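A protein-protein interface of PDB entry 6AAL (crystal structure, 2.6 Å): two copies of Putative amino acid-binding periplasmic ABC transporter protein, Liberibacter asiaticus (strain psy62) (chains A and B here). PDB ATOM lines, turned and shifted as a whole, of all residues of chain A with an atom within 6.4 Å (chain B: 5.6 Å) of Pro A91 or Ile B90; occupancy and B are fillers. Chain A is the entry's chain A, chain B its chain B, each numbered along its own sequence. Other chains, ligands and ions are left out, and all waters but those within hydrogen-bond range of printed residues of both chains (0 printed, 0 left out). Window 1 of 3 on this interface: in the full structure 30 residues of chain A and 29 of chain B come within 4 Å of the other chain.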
ATOM      1  N   ILE A  78      12.351  11.849  20.234  1.00  0.00           N
ATOM      2  CA  ILE A  78      10.923  11.578  20.272  1.00  0.00           C
ATOM      3  C   ILE A  78      10.647  10.125  20.510  1.00  0.00           C
ATOM      4  O   ILE A  78      11.060   9.282  19.743  1.00  0.00           O
ATOM      5  CB  ILE A  78      10.265  11.962  18.934  1.00  0.00           C
ATOM      6  CG1 ILE A  78      10.425  13.483  18.668  1.00  0.00           C
ATOM      7  CG2 ILE A  78       8.817  11.503  18.913  1.00  0.00           C
ATOM      8  CD1 ILE A  78       9.802  13.994  17.392  1.00  0.00           C
ATOM      9  N   GLN A  83       5.587  11.352  23.607  1.00  0.00           N
ATOM     10  CA  GLN A  83       4.593  12.009  22.779  1.00  0.00           C
ATOM     11  C   GLN A  83       3.247  12.092  23.501  1.00  0.00           C
ATOM     12  O   GLN A  83       2.597  13.129  23.444  1.00  0.00           O
ATOM     13  CB  GLN A  83       4.484  11.341  21.408  1.00  0.00           C
ATOM     14  CG  GLN A  83       4.184  12.327  20.274  1.00  0.00           C
ATOM     15  CD  GLN A  83       5.113  12.184  19.061  1.00  0.00           C
ATOM     16  OE1 GLN A  83       5.533  11.072  18.707  1.00  0.00           O
ATOM     17  NE2 GLN A  83       5.419  13.319  18.403  1.00  0.00           N
ATOM     18  N   SER A  89       8.193  19.823  19.304  1.00  0.00           N
ATOM     19  CA  SER A  89       8.273  20.528  18.022  1.00  0.00           C
ATOM     20  C   SER A  89       8.452  19.550  16.863  1.00  0.00           C
ATOM     21  O   SER A  89       8.778  18.370  17.017  1.00  0.00           O
ATOM     22  CB  SER A  89       9.443  21.529  18.005  1.00  0.00           C
ATOM     23  OG  SER A  89      10.738  20.909  18.023  1.00  0.00           O
ATOM     24  N   ILE A  90       8.247  20.081  15.679  1.00  0.00           N
ATOM     25  CA  ILE A  90       8.782  19.485  14.481  1.00  0.00           C
ATOM     26  C   ILE A  90      10.226  19.056  14.748  1.00  0.00           C
ATOM     27  O   ILE A  90      10.995  19.767  15.406  1.00  0.00           O
ATOM     28  CB  ILE A  90       8.749  20.503  13.332  1.00  0.00           C
ATOM     29  CG1 ILE A  90       9.099  19.830  12.029  1.00  0.00           C
ATOM     30  CG2 ILE A  90       9.647  21.705  13.607  1.00  0.00           C
ATOM     31  CD1 ILE A  90       7.860  19.619  11.203  1.00  0.00           C
ATOM     32  N   PRO A  91      10.602  17.888  14.264  1.00  0.00           N
ATOM     33  CA  PRO A  91      11.984  17.555  14.370  1.00  0.00           C
ATOM     34  C   PRO A  91      12.904  18.584  13.718  1.00  0.00           C
ATOM     35  O   PRO A  91      12.526  19.250  12.729  1.00  0.00           O
ATOM     36  CB  PRO A  91      12.056  16.231  13.616  1.00  0.00           C
ATOM     37  CG  PRO A  91      10.739  15.593  13.957  1.00  0.00           C
ATOM     38  CD  PRO A  91       9.771  16.727  13.923  1.00  0.00           C
ATOM     39  N   TYR A  92      14.109  18.705  14.274  1.00  0.00           N
ATOM     40  CA  TYR A  92      15.126  19.599  13.727  1.00  0.00           C
ATOM     41  C   TYR A  92      16.464  18.937  13.418  1.00  0.00           C
ATOM     42  O   TYR A  92      17.309  19.522  12.733  1.00  0.00           O
ATOM     43  CB  TYR A  92      15.328  20.830  14.625  1.00  0.00           C
ATOM     44  CG  TYR A  92      15.928  20.645  16.011  1.00  0.00           C
ATOM     45  CD1 TYR A  92      17.320  20.492  16.196  1.00  0.00           C
ATOM     46  CD2 TYR A  92      15.144  20.753  17.144  1.00  0.00           C
ATOM     47  CE1 TYR A  92      17.885  20.397  17.468  1.00  0.00           C
ATOM     48  CE2 TYR A  92      15.704  20.661  18.418  1.00  0.00           C
ATOM     49  CZ  TYR A  92      17.070  20.489  18.574  1.00  0.00           C
ATOM     50  OH  TYR A  92      17.607  20.395  19.842  1.00  0.00           O
ATOM     51  N   ILE A  93      16.644  17.715  13.908  1.00  0.00           N
ATOM     52  CA  ILE A  93      17.851  16.982  13.677  1.00  0.00           C
ATOM     53  C   ILE A  93      17.498  15.529  13.838  1.00  0.00           C
ATOM     54  O   ILE A  93      16.435  15.197  14.363  1.00  0.00           O
ATOM     55  CB  ILE A  93      18.966  17.464  14.660  1.00  0.00           C
ATOM     56  CG1 ILE A  93      20.353  16.934  14.274  1.00  0.00           C
ATOM     57  CG2 ILE A  93      18.677  17.069  16.119  1.00  0.00           C
ATOM     58  CD1 ILE A  93      20.717  17.150  12.830  1.00  0.00           C
ATOM     59  N   ALA A 191      14.513  10.746  15.285  1.00  0.00           N
ATOM     60  CA  ALA A 191      14.239  12.168  15.305  1.00  0.00           C
ATOM     61  C   ALA A 191      14.419  12.754  16.691  1.00  0.00           C
ATOM     62  O   ALA A 191      14.148  12.109  17.736  1.00  0.00           O
ATOM     63  CB  ALA A 191      12.838  12.483  14.808  1.00  0.00           C
ATOM     64  N   VAL A 192      14.898  13.996  16.651  1.00  0.00           N
ATOM     65  CA  VAL A 192      15.142  14.796  17.811  1.00  0.00           C
ATOM     66  C   VAL A 192      14.393  16.132  17.631  1.00  0.00           C
ATOM     67  O   VAL A 192      14.250  16.622  16.503  1.00  0.00           O
ATOM     68  CB  VAL A 192      16.645  14.991  17.957  1.00  0.00           C
ATOM     69  CG1 VAL A 192      16.944  15.980  19.072  1.00  0.00           C
ATOM     70  CG2 VAL A 192      17.334  13.625  18.170  1.00  0.00           C
ATOM     71  N   ALA A 193      13.883  16.670  18.740  1.00  0.00           N
ATOM     72  CA  ALA A 193      13.118  17.917  18.754  1.00  0.00           C
ATOM     73  C   ALA A 193      13.208  18.637  20.107  1.00  0.00           C
ATOM     74  O   ALA A 193      13.796  18.129  21.055  1.00  0.00           O
ATOM     75  CB  ALA A 193      11.659  17.637  18.421  1.00  0.00           C
ATOM     76  N   PHE A 194      12.614  19.831  20.162  1.00  0.00           N
ATOM     77  CA  PHE A 194      12.414  20.589  21.414  1.00  0.00           C
ATOM     78  C   PHE A 194      11.227  20.043  22.134  1.00  0.00           C
ATOM     79  O   PHE A 194      10.197  19.848  21.509  1.00  0.00           O
ATOM     80  CB  PHE A 194      12.161  22.059  21.100  1.00  0.00           C
ATOM     81  CG  PHE A 194      13.330  22.732  20.452  1.00  0.00           C
ATOM     82  CD1 PHE A 194      14.494  22.953  21.165  1.00  0.00           C
ATOM     83  CD2 PHE A 194      13.277  23.118  19.122  1.00  0.00           C
ATOM     84  CE1 PHE A 194      15.580  23.560  20.566  1.00  0.00           C
ATOM     85  CE2 PHE A 194      14.360  23.741  18.519  1.00  0.00           C
ATOM     86  CZ  PHE A 194      15.515  23.958  19.240  1.00  0.00           C
ATOM     87  N   ASN A 208       7.737  25.907  15.567  1.00  0.00           N
ATOM     88  CA  ASN A 208       7.642  25.182  14.306  1.00  0.00           C
ATOM     89  C   ASN A 208       7.612  26.124  13.126  1.00  0.00           C
ATOM     90  O   ASN A 208       8.206  25.847  12.094  1.00  0.00           O
ATOM     91  CB  ASN A 208       6.391  24.296  14.255  1.00  0.00           C
ATOM     92  CG  ASN A 208       6.446  23.109  15.227  1.00  0.00           C
ATOM     93  OD1 ASN A 208       7.465  22.866  15.903  1.00  0.00           O
ATOM     94  ND2 ASN A 208       5.317  22.363  15.317  1.00  0.00           N
ATOM     95  N   LEU A 211      11.121  27.606  12.829  1.00  0.00           N
ATOM     96  CA  LEU A 211      12.092  26.631  12.323  1.00  0.00           C
ATOM     97  C   LEU A 211      11.935  26.549  10.845  1.00  0.00           C
ATOM     98  O   LEU A 211      12.896  26.500  10.109  1.00  0.00           O
ATOM     99  CB  LEU A 211      11.896  25.250  12.910  1.00  0.00           C
ATOM    100  CG  LEU A 211      12.468  25.082  14.316  1.00  0.00           C
ATOM    101  CD1 LEU A 211      11.934  23.793  14.914  1.00  0.00           C
ATOM    102  CD2 LEU A 211      13.987  25.064  14.328  1.00  0.00           C
ATOM    103  N   HIS A 215      15.064  27.031   8.195  1.00  0.00           N
ATOM    104  CA  HIS A 215      15.311  26.288   6.945  1.00  0.00           C
ATOM    105  C   HIS A 215      15.218  27.127   5.666  1.00  0.00           C
ATOM    106  O   HIS A 215      16.155  27.165   4.869  1.00  0.00           O
ATOM    107  CB  HIS A 215      14.326  25.146   6.817  1.00  0.00           C
ATOM    108  CG  HIS A 215      14.725  23.932   7.584  1.00  0.00           C
ATOM    109  ND1 HIS A 215      14.097  23.546   8.750  1.00  0.00           N
ATOM    110  CD2 HIS A 215      15.695  23.019   7.348  1.00  0.00           C
ATOM    111  CE1 HIS A 215      14.665  22.440   9.196  1.00  0.00           C
ATOM    112  NE2 HIS A 215      15.633  22.098   8.361  1.00  0.00           N
ATOM    113  N   VAL A 236      17.191  16.894   8.883  1.00  0.00           N
ATOM    114  CA  VAL A 236      15.778  16.667   8.632  1.00  0.00           C
ATOM    115  C   VAL A 236      15.406  17.423   7.383  1.00  0.00           C
ATOM    116  O   VAL A 236      16.170  18.302   6.925  1.00  0.00           O
ATOM    117  CB  VAL A 236      14.921  17.126   9.841  1.00  0.00           C
ATOM    118  CG1 VAL A 236      15.528  16.593  11.145  1.00  0.00           C
ATOM    119  CG2 VAL A 236      14.799  18.643   9.901  1.00  0.00           C
ATOM    120  N   PRO A 237      14.251  17.085   6.805  1.00  0.00           N
ATOM    121  CA  PRO A 237      13.789  17.793   5.612  1.00  0.00           C
ATOM    122  C   PRO A 237      13.609  19.270   5.832  1.00  0.00           C
ATOM    123  O   PRO A 237      13.372  19.677   6.961  1.00  0.00           O
ATOM    124  CB  PRO A 237      12.433  17.140   5.294  1.00  0.00           C
ATOM    125  CG  PRO A 237      12.111  16.251   6.450  1.00  0.00           C
ATOM    126  CD  PRO A 237      13.442  15.883   7.053  1.00  0.00           C
ATOM    127  N   PHE B  88      -0.091  20.906  11.816  1.00  0.00           N
ATOM    128  CA  PHE B  88       0.565  19.847  11.046  1.00  0.00           C
ATOM    129  C   PHE B  88       0.931  18.664  11.918  1.00  0.00           C
ATOM    130  O   PHE B  88       1.147  18.785  13.103  1.00  0.00           O
ATOM    131  CB  PHE B  88       1.827  20.374  10.375  1.00  0.00           C
ATOM    132  CG  PHE B  88       1.559  21.149   9.145  1.00  0.00           C
ATOM    133  CD1 PHE B  88       1.632  22.550   9.156  1.00  0.00           C
ATOM    134  CD2 PHE B  88       1.202  20.497   7.993  1.00  0.00           C
ATOM    135  CE1 PHE B  88       1.370  23.269   8.003  1.00  0.00           C
ATOM    136  CE2 PHE B  88       0.938  21.210   6.837  1.00  0.00           C
ATOM    137  CZ  PHE B  88       1.022  22.599   6.834  1.00  0.00           C
ATOM    138  N   SER B  89       1.007  17.502  11.315  1.00  0.00           N
ATOM    139  CA  SER B  89       1.538  16.367  11.994  1.00  0.00           C
ATOM    140  C   SER B  89       3.051  16.482  11.880  1.00  0.00           C
ATOM    141  O   SER B  89       3.602  17.499  11.386  1.00  0.00           O
ATOM    142  CB  SER B  89       1.036  15.092  11.343  1.00  0.00           C
ATOM    143  OG  SER B  89       1.557  14.916  10.033  1.00  0.00           O
ATOM    144  N   ILE B  90       3.719  15.467  12.402  1.00  0.00           N
ATOM    145  CA  ILE B  90       5.118  15.325  12.186  1.00  0.00           C
ATOM    146  C   ILE B  90       5.247  14.985  10.690  1.00  0.00           C
ATOM    147  O   ILE B  90       4.367  14.287  10.123  1.00  0.00           O
ATOM    148  CB  ILE B  90       5.692  14.183  13.049  1.00  0.00           C
ATOM    149  CG1 ILE B  90       7.197  14.359  13.273  1.00  0.00           C
ATOM    150  CG2 ILE B  90       5.409  12.827  12.388  1.00  0.00           C
ATOM    151  CD1 ILE B  90       7.752  13.579  14.464  1.00  0.00           C
ATOM    152  N   PRO B  91       6.329  15.442  10.039  1.00  0.00           N
ATOM    153  CA  PRO B  91       6.461  15.049   8.644  1.00  0.00           C
ATOM    154  C   PRO B  91       6.594  13.530   8.484  1.00  0.00           C
ATOM    155  O   PRO B  91       7.282  12.874   9.279  1.00  0.00           O
ATOM    156  CB  PRO B  91       7.747  15.763   8.185  1.00  0.00           C
ATOM    157  CG  PRO B  91       7.925  16.851   9.160  1.00  0.00           C
ATOM    158  CD  PRO B  91       7.454  16.264  10.466  1.00  0.00           C
ATOM    159  N   TYR B  92       5.940  13.011   7.452  1.00  0.00           N
ATOM    160  CA  TYR B  92       5.944  11.588   7.130  1.00  0.00           C
ATOM    161  C   TYR B  92       6.550  11.227   5.766  1.00  0.00           C
ATOM    162  O   TYR B  92       6.640  10.053   5.432  1.00  0.00           O
ATOM    163  CB  TYR B  92       4.484  11.027   7.234  1.00  0.00           C
ATOM    164  CG  TYR B  92       3.429  11.485   6.182  1.00  0.00           C
ATOM    165  CD1 TYR B  92       3.304  10.844   4.948  1.00  0.00           C
ATOM    166  CD2 TYR B  92       2.539  12.490   6.462  1.00  0.00           C
ATOM    167  CE1 TYR B  92       2.351  11.233   4.029  1.00  0.00           C
ATOM    168  CE2 TYR B  92       1.585  12.893   5.540  1.00  0.00           C
ATOM    169  CZ  TYR B  92       1.499  12.270   4.328  1.00  0.00           C
ATOM    170  OH  TYR B  92       0.533  12.672   3.423  1.00  0.00           O
ATOM    171  N   VAL B 192       6.629  17.145   4.114  1.00  0.00           N
ATOM    172  CA  VAL B 192       5.207  16.967   3.799  1.00  0.00           C
ATOM    173  C   VAL B 192       4.543  16.219   4.965  1.00  0.00           C
ATOM    174  O   VAL B 192       5.158  15.346   5.588  1.00  0.00           O
ATOM    175  CB  VAL B 192       5.043  16.181   2.485  1.00  0.00           C
ATOM    176  CG1 VAL B 192       3.590  15.993   2.102  1.00  0.00           C
ATOM    177  CG2 VAL B 192       5.761  16.880   1.355  1.00  0.00           C
ATOM    178  N   ALA B 193       3.298  16.573   5.271  1.00  0.00           N
ATOM    179  CA  ALA B 193       2.620  16.093   6.490  1.00  0.00           C
ATOM    180  C   ALA B 193       1.089  16.147   6.376  1.00  0.00           C
ATOM    181  O   ALA B 193       0.532  16.580   5.348  1.00  0.00           O
ATOM    182  CB  ALA B 193       3.077  16.912   7.698  1.00  0.00           C
ATOM    183  N   PHE B 194       0.416  15.668   7.423  1.00  0.00           N
ATOM    184  CA  PHE B 194      -1.051  15.691   7.477  1.00  0.00           C
ATOM    185  C   PHE B 194      -1.500  17.029   8.043  1.00  0.00           C
ATOM    186  O   PHE B 194      -0.907  17.501   8.990  1.00  0.00           O
ATOM    187  CB  PHE B 194      -1.596  14.507   8.328  1.00  0.00           C
ATOM    188  CG  PHE B 194      -1.348  13.156   7.700  1.00  0.00           C
ATOM    189  CD1 PHE B 194      -2.054  12.762   6.574  1.00  0.00           C
ATOM    190  CD2 PHE B 194      -0.389  12.287   8.223  1.00  0.00           C
ATOM    191  CE1 PHE B 194      -1.803  11.526   5.994  1.00  0.00           C
ATOM    192  CE2 PHE B 194      -0.153  11.046   7.661  1.00  0.00           C
ATOM    193  CZ  PHE B 194      -0.856  10.670   6.541  1.00  0.00           C
ATOM    194  N   ASN B 208       0.763  11.671  15.567  1.00  0.00           N
ATOM    195  CA  ASN B 208       2.189  11.737  15.837  1.00  0.00           C
ATOM    196  C   ASN B 208       2.689  10.487  16.543  1.00  0.00           C
ATOM    197  O   ASN B 208       3.706   9.866  16.146  1.00  0.00           O
ATOM    198  CB  ASN B 208       2.491  13.001  16.631  1.00  0.00           C
ATOM    199  CG  ASN B 208       2.458  14.253  15.761  1.00  0.00           C
ATOM    200  OD1 ASN B 208       2.390  14.173  14.522  1.00  0.00           O
ATOM    201  ND2 ASN B 208       2.525  15.412  16.393  1.00  0.00           N
ATOM    202  N   LEU B 211       2.475   7.412  14.279  1.00  0.00           N
ATOM    203  CA  LEU B 211       3.517   7.510  13.244  1.00  0.00           C
ATOM    204  C   LEU B 211       4.860   7.100  13.822  1.00  0.00           C
ATOM    205  O   LEU B 211       5.659   6.417  13.194  1.00  0.00           O
ATOM    206  CB  LEU B 211       3.577   8.922  12.694  1.00  0.00           C
ATOM    207  CG  LEU B 211       2.482   9.236  11.667  1.00  0.00           C
ATOM    208  CD1 LEU B 211       2.618  10.642  11.165  1.00  0.00           C
ATOM    209  CD2 LEU B 211       2.555   8.291  10.472  1.00  0.00           C
ATOM    210  N   PRO B 237      12.891  10.887   9.279  1.00  0.00           N
ATOM    211  CA  PRO B 237      13.604  10.121  10.304  1.00  0.00           C
ATOM    212  C   PRO B 237      12.779   9.084  11.002  1.00  0.00           C
ATOM    213  O   PRO B 237      11.564   9.158  10.991  1.00  0.00           O
ATOM    214  CB  PRO B 237      13.983  11.183  11.311  1.00  0.00           C
ATOM    215  CG  PRO B 237      14.148  12.386  10.467  1.00  0.00           C
ATOM    216  CD  PRO B 237      12.979  12.318   9.544  1.00  0.00           C
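Ile A90 touches Pro B91, and with the chains exchanged Pro A91 touches Ile B90.
Pro A91 touches one residue of chain B.
Ile B90 touches just these residues of chain A: Ile A78 and Pro A91.
Printed residues of chain B within 4 Å of Ile A90: Pro B91.
Printed residues of chain A within 4 Å of Pro B91: Ile A90.
Of the printed residues of chain B, Ala A191 touches Pro B237 (3.9 Å).
Of the printed residues of chain B, Gln A83 touches Asn B208 (3.4 Å).
Of the printed residues of chain A, Asn B208 touches Gln A83.
Phe B88 touches none of the printed residues of chain A.
The nearest residue of chain B that does not touch Pro A91 is Pro B91 (4.2 Å).
The side-chain amide oxygen of Gln A83 lies close to the backbone carbonyl oxygen of Asn B208 (3.4 Å).
The backbone carbonyl oxygen (O) of Ala A191 lies within hydrogen-bond range of the backbone NH (N) of Ile A78.
N of Ile A90 sits at hydrogen-bond distance from OD1 of Asn A208, 2.9 Å away.
The side-chain amide oxygen (OD1) of Asn B208 sits at hydrogen-bond distance from the backbone NH (N) of Ile B90 (2.8 Å).
Hydrophobic or aromatic side chains of chain B within 4 Å of the printed part of chain A: Ile B90, Pro B91 and Pro B237.
Printed residues of chain A that touch a printed residue of chain B: Ile A78, Gln A83, Ile A90, Pro A91 and Ala A191.
Hydrophobic or aromatic side chains of chain A within 4 Å of the printed part of chain B: Ile A78, Ile A90, Pro A91 and Ala A191.
Among the printed residues, pairs that only touch across the chains: Ile A90 with Pro B91 (3.4 Å), Pro A91 with Ile B90 (3.6 Å), Ile A78 with Ile B90 (3.6 Å) and Ala A191 with Pro B237 (3.9 Å).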
